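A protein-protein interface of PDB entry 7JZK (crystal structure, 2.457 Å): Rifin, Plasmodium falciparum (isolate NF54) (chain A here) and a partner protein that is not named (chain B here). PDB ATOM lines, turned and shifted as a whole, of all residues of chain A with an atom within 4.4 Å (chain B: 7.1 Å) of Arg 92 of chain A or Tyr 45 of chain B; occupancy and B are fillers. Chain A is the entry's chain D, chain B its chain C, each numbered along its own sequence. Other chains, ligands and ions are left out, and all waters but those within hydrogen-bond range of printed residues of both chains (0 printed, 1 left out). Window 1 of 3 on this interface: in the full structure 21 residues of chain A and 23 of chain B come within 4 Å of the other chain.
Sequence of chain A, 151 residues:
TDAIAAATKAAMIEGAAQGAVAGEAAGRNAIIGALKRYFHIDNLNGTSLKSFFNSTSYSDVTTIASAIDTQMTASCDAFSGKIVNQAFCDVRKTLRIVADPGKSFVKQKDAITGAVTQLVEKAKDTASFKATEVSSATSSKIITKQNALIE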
ATOM      1  N   MET A  72       5.896   9.117  -8.458  1.00  0.00           N
ATOM      2  CA  MET A  72       5.672   9.401  -7.039  1.00  0.00           C
ATOM      3  C   MET A  72       6.952   9.215  -6.242  1.00  0.00           C
ATOM      4  O   MET A  72       7.253  10.008  -5.343  1.00  0.00           O
ATOM      5  CB  MET A  72       4.564   8.506  -6.476  1.00  0.00           C
ATOM      6  CG  MET A  72       4.197   8.769  -5.016  1.00  0.00           C
ATOM      7  SD  MET A  72       2.683   7.904  -4.500  1.00  0.00           S
ATOM      8  CE  MET A  72       1.513   8.938  -5.397  1.00  0.00           C
ATOM      9  N   THR A  73       7.715   8.158  -6.533  1.00  0.00           N
ATOM     10  CA  THR A  73       8.979   8.015  -5.822  1.00  0.00           C
ATOM     11  C   THR A  73       9.917   9.168  -6.162  1.00  0.00           C
ATOM     12  O   THR A  73      10.634   9.678  -5.285  1.00  0.00           O
ATOM     13  CB  THR A  73       9.623   6.657  -6.128  1.00  0.00           C
ATOM     14  OG1 THR A  73       8.744   5.620  -5.672  1.00  0.00           O
ATOM     15  CG2 THR A  73      10.973   6.499  -5.398  1.00  0.00           C
ATOM     16  N   CYS A  76       8.331  13.051  -4.613  1.00  0.00           N
ATOM     17  CA  CYS A  76       7.886  13.192  -3.233  1.00  0.00           C
ATOM     18  C   CYS A  76       8.951  12.666  -2.292  1.00  0.00           C
ATOM     19  O   CYS A  76       8.673  11.904  -1.367  1.00  0.00           O
ATOM     20  CB  CYS A  76       6.592  12.438  -2.990  1.00  0.00           C
ATOM     21  SG  CYS A  76       5.324  12.853  -4.152  1.00  0.00           S
ATOM     22  N   ASP A  77      10.193  13.081  -2.498  1.00  0.00           N
ATOM     23  CA  ASP A  77      11.317  12.523  -1.761  1.00  0.00           C
ATOM     24  C   ASP A  77      11.876  13.501  -0.732  1.00  0.00           C
ATOM     25  O   ASP A  77      11.536  14.688  -0.699  1.00  0.00           O
ATOM     26  CB  ASP A  77      12.446  12.102  -2.708  1.00  0.00           C
ATOM     27  CG  ASP A  77      13.052  13.272  -3.468  1.00  0.00           C
ATOM     28  OD1 ASP A  77      12.317  14.037  -4.143  1.00  0.00           O
ATOM     29  OD2 ASP A  77      14.277  13.471  -3.321  1.00  0.00           O
ATOM     30  N   ALA A  78      12.778  12.971   0.111  1.00  0.00           N
ATOM     31  CA  ALA A  78      13.381  13.760   1.173  1.00  0.00           C
ATOM     32  C   ALA A  78      14.561  14.591   0.677  1.00  0.00           C
ATOM     33  O   ALA A  78      14.925  15.571   1.331  1.00  0.00           O
ATOM     34  CB  ALA A  78      13.814  12.832   2.330  1.00  0.00           C
ATOM     35  N   CYS A  89       1.645  13.981  -3.744  1.00  0.00           N
ATOM     36  CA  CYS A  89       2.279  13.228  -2.671  1.00  0.00           C
ATOM     37  C   CYS A  89       1.278  12.896  -1.570  1.00  0.00           C
ATOM     38  O   CYS A  89       1.318  11.798  -1.012  1.00  0.00           O
ATOM     39  CB  CYS A  89       3.455  14.051  -2.132  1.00  0.00           C
ATOM     40  SG  CYS A  89       4.544  14.599  -3.478  1.00  0.00           S
ATOM     41  N   ASP A  90       0.296  13.763  -1.361  1.00  0.00           N
ATOM     42  CA  ASP A  90      -0.741  13.588  -0.345  1.00  0.00           C
ATOM     43  C   ASP A  90      -1.547  12.310  -0.571  1.00  0.00           C
ATOM     44  O   ASP A  90      -2.120  11.774   0.383  1.00  0.00           O
ATOM     45  CB  ASP A  90      -1.657  14.834  -0.353  1.00  0.00           C
ATOM     46  CG  ASP A  90      -2.774  14.786   0.706  1.00  0.00           C
ATOM     47  OD1 ASP A  90      -3.920  14.428   0.357  1.00  0.00           O
ATOM     48  OD2 ASP A  90      -2.506  15.106   1.891  1.00  0.00           O
ATOM     49  N   VAL A  91      -1.557  11.788  -1.804  1.00  0.00           N
ATOM     50  CA  VAL A  91      -2.250  10.540  -2.117  1.00  0.00           C
ATOM     51  C   VAL A  91      -1.694   9.377  -1.309  1.00  0.00           C
ATOM     52  O   VAL A  91      -2.422   8.423  -0.999  1.00  0.00           O
ATOM     53  CB  VAL A  91      -2.173  10.260  -3.629  1.00  0.00           C
ATOM     54  CG1 VAL A  91      -2.841   8.915  -3.986  1.00  0.00           C
ATOM     55  CG2 VAL A  91      -2.837  11.381  -4.372  1.00  0.00           C
ATOM     56  N   ARG A  92      -0.420   9.446  -0.919  1.00  0.00           N
ATOM     57  CA  ARG A  92       0.139   8.404  -0.060  1.00  0.00           C
ATOM     58  C   ARG A  92      -0.655   8.264   1.230  1.00  0.00           C
ATOM     59  O   ARG A  92      -0.712   7.176   1.813  1.00  0.00           O
ATOM     60  CB  ARG A  92       1.600   8.711   0.246  1.00  0.00           C
ATOM     61  CG  ARG A  92       2.527   8.292  -0.847  1.00  0.00           C
ATOM     62  CD  ARG A  92       3.896   8.789  -0.539  1.00  0.00           C
ATOM     63  NE  ARG A  92       4.871   8.293  -1.493  1.00  0.00           N
ATOM     64  CZ  ARG A  92       6.116   8.730  -1.528  1.00  0.00           C
ATOM     65  NH1 ARG A  92       6.489   9.661  -0.669  1.00  0.00           N
ATOM     66  NH2 ARG A  92       6.978   8.247  -2.412  1.00  0.00           N
ATOM     67  N   LYS A  93      -1.245   9.362   1.710  1.00  0.00           N
ATOM     68  CA  LYS A  93      -2.062   9.279   2.910  1.00  0.00           C
ATOM     69  C   LYS A  93      -3.402   8.632   2.616  1.00  0.00           C
ATOM     70  O   LYS A  93      -3.884   7.817   3.409  1.00  0.00           O
ATOM     71  CB  LYS A  93      -2.245  10.678   3.501  1.00  0.00           C
ATOM     72  CG  LYS A  93      -3.341  10.826   4.548  1.00  0.00           C
ATOM     73  CD  LYS A  93      -4.706  11.266   3.952  1.00  0.00           C
ATOM     74  CE  LYS A  93      -4.525  12.396   2.917  1.00  0.00           C
ATOM     75  NZ  LYS A  93      -5.649  12.661   1.944  1.00  0.00           N
ATOM     76  N   THR A  94      -3.951   8.883   1.437  1.00  0.00           N
ATOM     77  CA  THR A  94      -5.200   8.246   1.059  1.00  0.00           C
ATOM     78  C   THR A  94      -5.017   6.738   0.931  1.00  0.00           C
ATOM     79  O   THR A  94      -5.829   5.960   1.434  1.00  0.00           O
ATOM     80  CB  THR A  94      -5.684   8.852  -0.258  1.00  0.00           C
ATOM     81  OG1 THR A  94      -5.712  10.285  -0.139  1.00  0.00           O
ATOM     82  CG2 THR A  94      -7.074   8.341  -0.602  1.00  0.00           C
ATOM     83  N   LEU A  95      -3.939   6.303   0.291  1.00  0.00           N
ATOM     84  CA  LEU A  95      -3.708   4.877   0.087  1.00  0.00           C
ATOM     85  C   LEU A  95      -3.042   4.193   1.273  1.00  0.00           C
ATOM     86  O   LEU A  95      -2.506   3.098   1.082  1.00  0.00           O
ATOM     87  CB  LEU A  95      -2.870   4.653  -1.180  1.00  0.00           C
ATOM     88  CG  LEU A  95      -3.472   5.267  -2.455  1.00  0.00           C
ATOM     89  CD1 LEU A  95      -2.631   4.990  -3.691  1.00  0.00           C
ATOM     90  CD2 LEU A  95      -4.884   4.745  -2.628  1.00  0.00           C
ATOM     91  N   ARG A  96      -3.016   4.838   2.451  1.00  0.00           N
ATOM     92  CA  ARG A  96      -2.362   4.325   3.658  1.00  0.00           C
ATOM     93  C   ARG A  96      -0.949   3.841   3.344  1.00  0.00           C
ATOM     94  O   ARG A  96      -0.518   2.762   3.759  1.00  0.00           O
ATOM     95  CB  ARG A  96      -3.195   3.241   4.359  1.00  0.00           C
ATOM     96  CG  ARG A  96      -4.427   3.788   5.095  1.00  0.00           C
ATOM     97  CD  ARG A  96      -5.663   2.943   4.840  1.00  0.00           C
ATOM     98  NE  ARG A  96      -6.096   3.067   3.450  1.00  0.00           N
ATOM     99  CZ  ARG A  96      -7.196   2.513   2.950  1.00  0.00           C
ATOM    100  NH1 ARG A  96      -7.502   2.688   1.666  1.00  0.00           N
ATOM    101  NH2 ARG A  96      -7.986   1.786   3.731  1.00  0.00           N
ATOM    102  N   ILE A  97      -0.213   4.670   2.607  1.00  0.00           N
ATOM    103  CA  ILE A  97       1.171   4.360   2.270  1.00  0.00           C
ATOM    104  C   ILE A  97       2.141   5.008   3.253  1.00  0.00           C
ATOM    105  O   ILE A  97       3.296   4.562   3.363  1.00  0.00           O
ATOM    106  CB  ILE A  97       1.491   4.799   0.824  1.00  0.00           C
ATOM    107  CG1 ILE A  97       0.533   4.159  -0.169  1.00  0.00           C
ATOM    108  CG2 ILE A  97       2.893   4.413   0.416  1.00  0.00           C
ATOM    109  CD1 ILE A  97       0.844   4.589  -1.589  1.00  0.00           C
ATOM    110  N   VAL A  98       1.701   6.021   3.995  1.00  0.00           N
ATOM    111  CA  VAL A  98       2.600   6.676   4.927  1.00  0.00           C
ATOM    112  C   VAL A  98       2.825   5.742   6.102  1.00  0.00           C
ATOM    113  O   VAL A  98       1.962   4.928   6.451  1.00  0.00           O
ATOM    114  CB  VAL A  98       2.016   8.030   5.373  1.00  0.00           C
ATOM    115  CG1 VAL A  98       1.802   8.931   4.167  1.00  0.00           C
ATOM    116  CG2 VAL A  98       0.686   7.818   6.057  1.00  0.00           C
ATOM    117  N   GLN A 108       3.844   0.897  -2.083  1.00  0.00           N
ATOM    118  CA  GLN A 108       3.267   1.989  -2.854  1.00  0.00           C
ATOM    119  C   GLN A 108       2.767   1.515  -4.211  1.00  0.00           C
ATOM    120  O   GLN A 108       1.652   1.831  -4.618  1.00  0.00           O
ATOM    121  CB  GLN A 108       4.335   3.081  -3.003  1.00  0.00           C
ATOM    122  CG  GLN A 108       4.028   4.231  -3.944  1.00  0.00           C
ATOM    123  CD  GLN A 108       5.139   5.285  -3.951  1.00  0.00           C
ATOM    124  OE1 GLN A 108       5.207   6.152  -3.088  1.00  0.00           O
ATOM    125  NE2 GLN A 108       6.073   5.146  -4.892  1.00  0.00           N
ATOM    126  N   ARG B  36      13.339   4.947   6.665  1.00  0.00           N
ATOM    127  CA  ARG B  36      12.631   5.975   5.909  1.00  0.00           C
ATOM    128  C   ARG B  36      12.903   7.330   6.545  1.00  0.00           C
ATOM    129  O   ARG B  36      12.634   7.528   7.743  1.00  0.00           O
ATOM    130  CB  ARG B  36      11.128   5.704   5.885  1.00  0.00           C
ATOM    131  CG  ARG B  36      10.235   6.876   5.526  1.00  0.00           C
ATOM    132  CD  ARG B  36       8.801   6.395   5.287  1.00  0.00           C
ATOM    133  NE  ARG B  36       8.725   5.338   4.279  1.00  0.00           N
ATOM    134  CZ  ARG B  36       7.592   4.741   3.902  1.00  0.00           C
ATOM    135  NH1 ARG B  36       6.430   5.092   4.452  1.00  0.00           N
ATOM    136  NH2 ARG B  36       7.615   3.791   2.973  1.00  0.00           N
ATOM    137  N   LEU B  37      13.392   8.264   5.729  1.00  0.00           N
ATOM    138  CA  LEU B  37      13.682   9.629   6.136  1.00  0.00           C
ATOM    139  C   LEU B  37      12.533  10.508   5.682  1.00  0.00           C
ATOM    140  O   LEU B  37      12.243  10.569   4.481  1.00  0.00           O
ATOM    141  CB  LEU B  37      14.999  10.106   5.544  1.00  0.00           C
ATOM    142  CG  LEU B  37      15.304  11.582   5.721  1.00  0.00           C
ATOM    143  CD1 LEU B  37      15.757  11.860   7.157  1.00  0.00           C
ATOM    144  CD2 LEU B  37      16.422  11.905   4.746  1.00  0.00           C
ATOM    145  N   GLU B  38      11.849  11.078   6.658  1.00  0.00           N
ATOM    146  CA  GLU B  38      10.640  11.858   6.371  1.00  0.00           C
ATOM    147  C   GLU B  38      10.914  13.340   6.524  1.00  0.00           C
ATOM    148  O   GLU B  38      11.793  13.704   7.284  1.00  0.00           O
ATOM    149  CB  GLU B  38       9.531  11.456   7.333  1.00  0.00           C
ATOM    150  CG  GLU B  38       8.838  10.148   7.041  1.00  0.00           C
ATOM    151  CD  GLU B  38       7.706   9.914   8.022  1.00  0.00           C
ATOM    152  OE1 GLU B  38       7.123   8.832   8.012  1.00  0.00           O
ATOM    153  OE2 GLU B  38       7.415  10.828   8.792  1.00  0.00           O
ATOM    154  N   ARG B  39      10.174  14.146   5.786  1.00  0.00           N
ATOM    155  CA  ARG B  39      10.262  15.607   5.939  1.00  0.00           C
ATOM    156  C   ARG B  39       9.210  16.041   6.951  1.00  0.00           C
ATOM    157  O   ARG B  39       8.701  15.200   7.667  1.00  0.00           O
ATOM    158  CB  ARG B  39      10.074  16.284   4.585  1.00  0.00           C
ATOM    159  CG  ARG B  39      11.150  15.958   3.564  1.00  0.00           C
ATOM    160  CD  ARG B  39      11.700  17.238   2.977  1.00  0.00           C
ATOM    161  NE  ARG B  39      12.196  18.116   4.024  1.00  0.00           N
ATOM    162  CZ  ARG B  39      12.746  19.302   3.817  1.00  0.00           C
ATOM    163  NH1 ARG B  39      12.885  19.770   2.591  1.00  0.00           N
ATOM    164  NH2 ARG B  39      13.155  20.019   4.843  1.00  0.00           N
ATOM    165  N   ARG B  41       6.340  16.621   6.411  1.00  0.00           N
ATOM    166  CA  ARG B  41       5.120  15.872   6.087  1.00  0.00           C
ATOM    167  C   ARG B  41       5.397  14.394   5.854  1.00  0.00           C
ATOM    168  O   ARG B  41       6.411  14.084   5.232  1.00  0.00           O
ATOM    169  CB  ARG B  41       4.264  16.624   5.072  1.00  0.00           C
ATOM    170  CG  ARG B  41       3.441  17.740   5.695  1.00  0.00           C
ATOM    171  CD  ARG B  41       3.276  18.938   4.787  1.00  0.00           C
ATOM    172  NE  ARG B  41       4.531  19.389   4.212  1.00  0.00           N
ATOM    173  CZ  ARG B  41       4.652  20.457   3.434  1.00  0.00           C
ATOM    174  NH1 ARG B  41       5.833  20.796   2.947  1.00  0.00           N
ATOM    175  NH2 ARG B  41       3.588  21.181   3.144  1.00  0.00           N
ATOM    176  N   ASN B  42       4.490  13.541   6.319  1.00  0.00           N
ATOM    177  CA  ASN B  42       4.605  12.063   6.275  1.00  0.00           C
ATOM    178  C   ASN B  42       4.729  11.567   4.847  1.00  0.00           C
ATOM    179  O   ASN B  42       5.370  10.546   4.653  1.00  0.00           O
ATOM    180  CB  ASN B  42       3.278  11.488   6.779  1.00  0.00           C
ATOM    181  CG  ASN B  42       3.374  10.672   8.043  1.00  0.00           C
ATOM    182  OD1 ASN B  42       4.462  10.405   8.536  1.00  0.00           O
ATOM    183  ND2 ASN B  42       2.231  10.271   8.572  1.00  0.00           N
ATOM    184  N   TYR B  43       4.072  12.235   3.918  1.00  0.00           N
ATOM    185  CA  TYR B  43       4.044  11.797   2.505  1.00  0.00           C
ATOM    186  C   TYR B  43       5.288  12.197   1.719  1.00  0.00           C
ATOM    187  O   TYR B  43       5.398  11.789   0.583  1.00  0.00           O
ATOM    188  CB  TYR B  43       2.731  12.249   1.872  1.00  0.00           C
ATOM    189  CG  TYR B  43       2.347  13.692   2.080  1.00  0.00           C
ATOM    190  CD1 TYR B  43       1.459  14.054   3.077  1.00  0.00           C
ATOM    191  CD2 TYR B  43       2.837  14.687   1.257  1.00  0.00           C
ATOM    192  CE1 TYR B  43       1.087  15.372   3.264  1.00  0.00           C
ATOM    193  CE2 TYR B  43       2.475  16.010   1.428  1.00  0.00           C
ATOM    194  CZ  TYR B  43       1.596  16.352   2.436  1.00  0.00           C
ATOM    195  OH  TYR B  43       1.232  17.649   2.617  1.00  0.00           O
ATOM    196  N   LEU B  44       6.144  13.022   2.287  1.00  0.00           N
ATOM    197  CA  LEU B  44       7.410  13.379   1.618  1.00  0.00           C
ATOM    198  C   LEU B  44       8.510  12.565   2.290  1.00  0.00           C
ATOM    199  O   LEU B  44       8.845  12.853   3.437  1.00  0.00           O
ATOM    200  CB  LEU B  44       7.605  14.886   1.742  1.00  0.00           C
ATOM    201  CG  LEU B  44       6.426  15.739   1.292  1.00  0.00           C
ATOM    202  CD1 LEU B  44       6.634  17.190   1.685  1.00  0.00           C
ATOM    203  CD2 LEU B  44       6.219  15.619  -0.205  1.00  0.00           C
ATOM    204  N   TYR B  45       8.987  11.532   1.603  1.00  0.00           N
ATOM    205  CA  TYR B  45       9.946  10.608   2.243  1.00  0.00           C
ATOM    206  C   TYR B  45      10.911   9.936   1.273  1.00  0.00           C
ATOM    207  O   TYR B  45      10.622   9.891   0.084  1.00  0.00           O
ATOM    208  CB  TYR B  45       9.182   9.583   3.084  1.00  0.00           C
ATOM    209  CG  TYR B  45       8.269   8.605   2.399  1.00  0.00           C
ATOM    210  CD1 TYR B  45       6.905   8.654   2.612  1.00  0.00           C
ATOM    211  CD2 TYR B  45       8.767   7.577   1.622  1.00  0.00           C
ATOM    212  CE1 TYR B  45       6.053   7.736   2.029  1.00  0.00           C
ATOM    213  CE2 TYR B  45       7.930   6.661   1.018  1.00  0.00           C
ATOM    214  CZ  TYR B  45       6.568   6.739   1.226  1.00  0.00           C
ATOM    215  OH  TYR B  45       5.746   5.832   0.643  1.00  0.00           O
ATOM    216  N   SER B  46      12.017   9.410   1.794  1.00  0.00           N
ATOM    217  CA  SER B  46      12.921   8.591   0.995  1.00  0.00           C
ATOM    218  C   SER B  46      13.283   7.359   1.804  1.00  0.00           C
ATOM    219  O   SER B  46      13.628   7.464   2.990  1.00  0.00           O
ATOM    220  CB  SER B  46      14.174   9.366   0.610  1.00  0.00           C
ATOM    221  OG  SER B  46      13.875  10.301  -0.420  1.00  0.00           O
ATOM    222  N   ASP B  47      13.214   6.200   1.163  1.00  0.00           N
ATOM    223  CA  ASP B  47      13.475   4.919   1.797  1.00  0.00           C
ATOM    224  C   ASP B  47      14.834   4.383   1.362  1.00  0.00           C
ATOM    225  O   ASP B  47      15.320   4.686   0.270  1.00  0.00           O
ATOM    226  CB  ASP B  47      12.374   3.914   1.448  1.00  0.00           C
ATOM    227  CG  ASP B  47      11.141   4.064   2.337  1.00  0.00           C
ATOM    228  OD1 ASP B  47      11.123   4.999   3.151  1.00  0.00           O
ATOM    229  OD2 ASP B  47      10.160   3.297   2.189  1.00  0.00           O
ATOM    230  N   PHE B  63      21.510   9.268   4.513  1.00  0.00           N
ATOM    231  CA  PHE B  63      20.854   9.965   3.404  1.00  0.00           C
ATOM    232  C   PHE B  63      21.640  11.246   3.191  1.00  0.00           C
ATOM    233  O   PHE B  63      21.658  12.107   4.076  1.00  0.00           O
ATOM    234  CB  PHE B  63      19.386  10.284   3.713  1.00  0.00           C
ATOM    235  CG  PHE B  63      18.574   9.093   4.159  1.00  0.00           C
ATOM    236  CD1 PHE B  63      18.626   8.649   5.479  1.00  0.00           C
ATOM    237  CD2 PHE B  63      17.743   8.428   3.272  1.00  0.00           C
ATOM    238  CE1 PHE B  63      17.891   7.568   5.886  1.00  0.00           C
ATOM    239  CE2 PHE B  63      17.002   7.340   3.690  1.00  0.00           C
ATOM    240  CZ  PHE B  63      17.081   6.917   5.001  1.00  0.00           C
ATOM    241  N   TRP B  86       6.232  -0.830  11.629  1.00  0.00           N
ATOM    242  CA  TRP B  86       6.967   0.414  11.660  1.00  0.00           C
ATOM    243  C   TRP B  86       7.233   0.746  13.119  1.00  0.00           C
ATOM    244  O   TRP B  86       6.374   0.538  13.976  1.00  0.00           O
ATOM    245  CB  TRP B  86       6.149   1.538  11.015  1.00  0.00           C
ATOM    246  CG  TRP B  86       6.157   1.534   9.538  1.00  0.00           C
ATOM    247  CD1 TRP B  86       5.105   1.242   8.713  1.00  0.00           C
ATOM    248  CD2 TRP B  86       7.248   1.889   8.691  1.00  0.00           C
ATOM    249  NE1 TRP B  86       5.489   1.364   7.401  1.00  0.00           N
ATOM    250  CE2 TRP B  86       6.799   1.767   7.360  1.00  0.00           C
ATOM    251  CE3 TRP B  86       8.563   2.290   8.927  1.00  0.00           C
ATOM    252  CZ2 TRP B  86       7.624   2.027   6.267  1.00  0.00           C
ATOM    253  CZ3 TRP B  86       9.384   2.546   7.842  1.00  0.00           C
ATOM    254  CH2 TRP B  86       8.910   2.415   6.532  1.00  0.00           C
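The side-chain amino group (NZ) of Lys 93 of chain A is in salt-bridge range of the side-chain carboxylate (OD1) of Asp 90 of chain A (2.9 Å). The backbone carbonyl oxygen of Met 72 of chain A is in hydrogen-bond range of the guanidinium group of Arg 92 of chain A (3.4 Å). OD1 of Asn 42 of chain B sits close to OE2 of Glu 38 of chain B, at 3.0 Å. The side-chain hydroxyl of Thr 73 of chain A sits at hydrogen-bond distance from the side-chain amide nitrogen of Gln 108 of chain A, at 2.8 Å. The backbone carbonyl oxygen (O) of Arg 92 of chain A is in hydrogen-bond range of the backbone NH (N) of Val 98 of chain A (3.5 Å). NE of Arg 36 of chain B lies within salt-bridge range of OD1 of Asp 47 of chain B (2.7 Å).
O of Cys 76 of chain A touches O of Tyr 43 of chain B, 3.8 Å away. Cys 76 of chain A touches Leu 44 of chain B. Asp 77 of chain A touches Tyr 45 of chain B (CA to O, 3.3 Å). Ser 46 of chain B touches Asp 77 of chain A. Leu 37 of chain B touches Ala 78 of chain A. Ala 78 of chain A touches Arg 39 of chain B (CA to CG, 3.9 Å). Ala 78 of chain A touches Tyr 45 of chain B (N to C, 3.7 Å). Asp 90 of chain A touches Tyr 43 of chain B. Ile 97 of chain A touches Tyr 45 of chain B. ND2 of Asn 42 of chain B touches CG2 of Val 98 of chain A, 3.8 Å away.
Printed residues of chain B that touch a printed residue of chain A: Arg 36, Leu 37, Arg 39, Asn 42, Tyr 43, Leu 44, Tyr 45 and Ser 46. Hydrophobic or aromatic side chains of chain B that line the printed part of chain A: Leu 37, Tyr 43, Leu 44 and Tyr 45. Printed residues of chain A that touch a printed residue of chain B: Cys 76, Asp 77, Ala 78, Cys 89, Asp 90, Arg 92, Ile 97, Val 98 and Gln 108. Among the printed residues, no Asp or Glu carboxylate lies within 4 Å of a Lys or Arg side-chain nitrogen of the other chain.
Printed residues of chain B within 4 Å of Asp 90 of chain A: Tyr 43. Of chain B, only Tyr 43 (2.7 Å) and Tyr 45 (3.3 Å) come within 4 Å of Arg 92 of chain A. Of the printed residues of chain B, Gln 108 of chain A touches Tyr 45. Of chain A, only Cys 76, Asp 77, Ala 78, Arg 92, Ile 97 and Gln 108 come within 4 Å of Tyr 45 of chain B. The nearest printed residue of chain A that does not touch Leu 44 of chain B is Arg 92 of chain A (4.5 Å).
The backbone carbonyl oxygen of Ile 97 of chain A lies within hydrogen-bond range of the guanidinium group of Arg 36 of chain B, at 3.4 Å. The side-chain hydroxyl of Tyr 45 of chain B lies within hydrogen-bond range of the guanidinium group of Arg 92 of chain A (3.4 Å). O of Tyr 43 of chain B lies within hydrogen-bond range of NH1 of Arg 92 of chain A (2.7 Å). O of Cys 76 of chain A sits at hydrogen-bond distance from N of Tyr 45 of chain B, at 3.0 Å. The backbone NH (N) of Ala 78 of chain A sits at hydrogen-bond distance from the side-chain hydroxyl (OG) of Ser 46 of chain B, at 2.9 Å.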
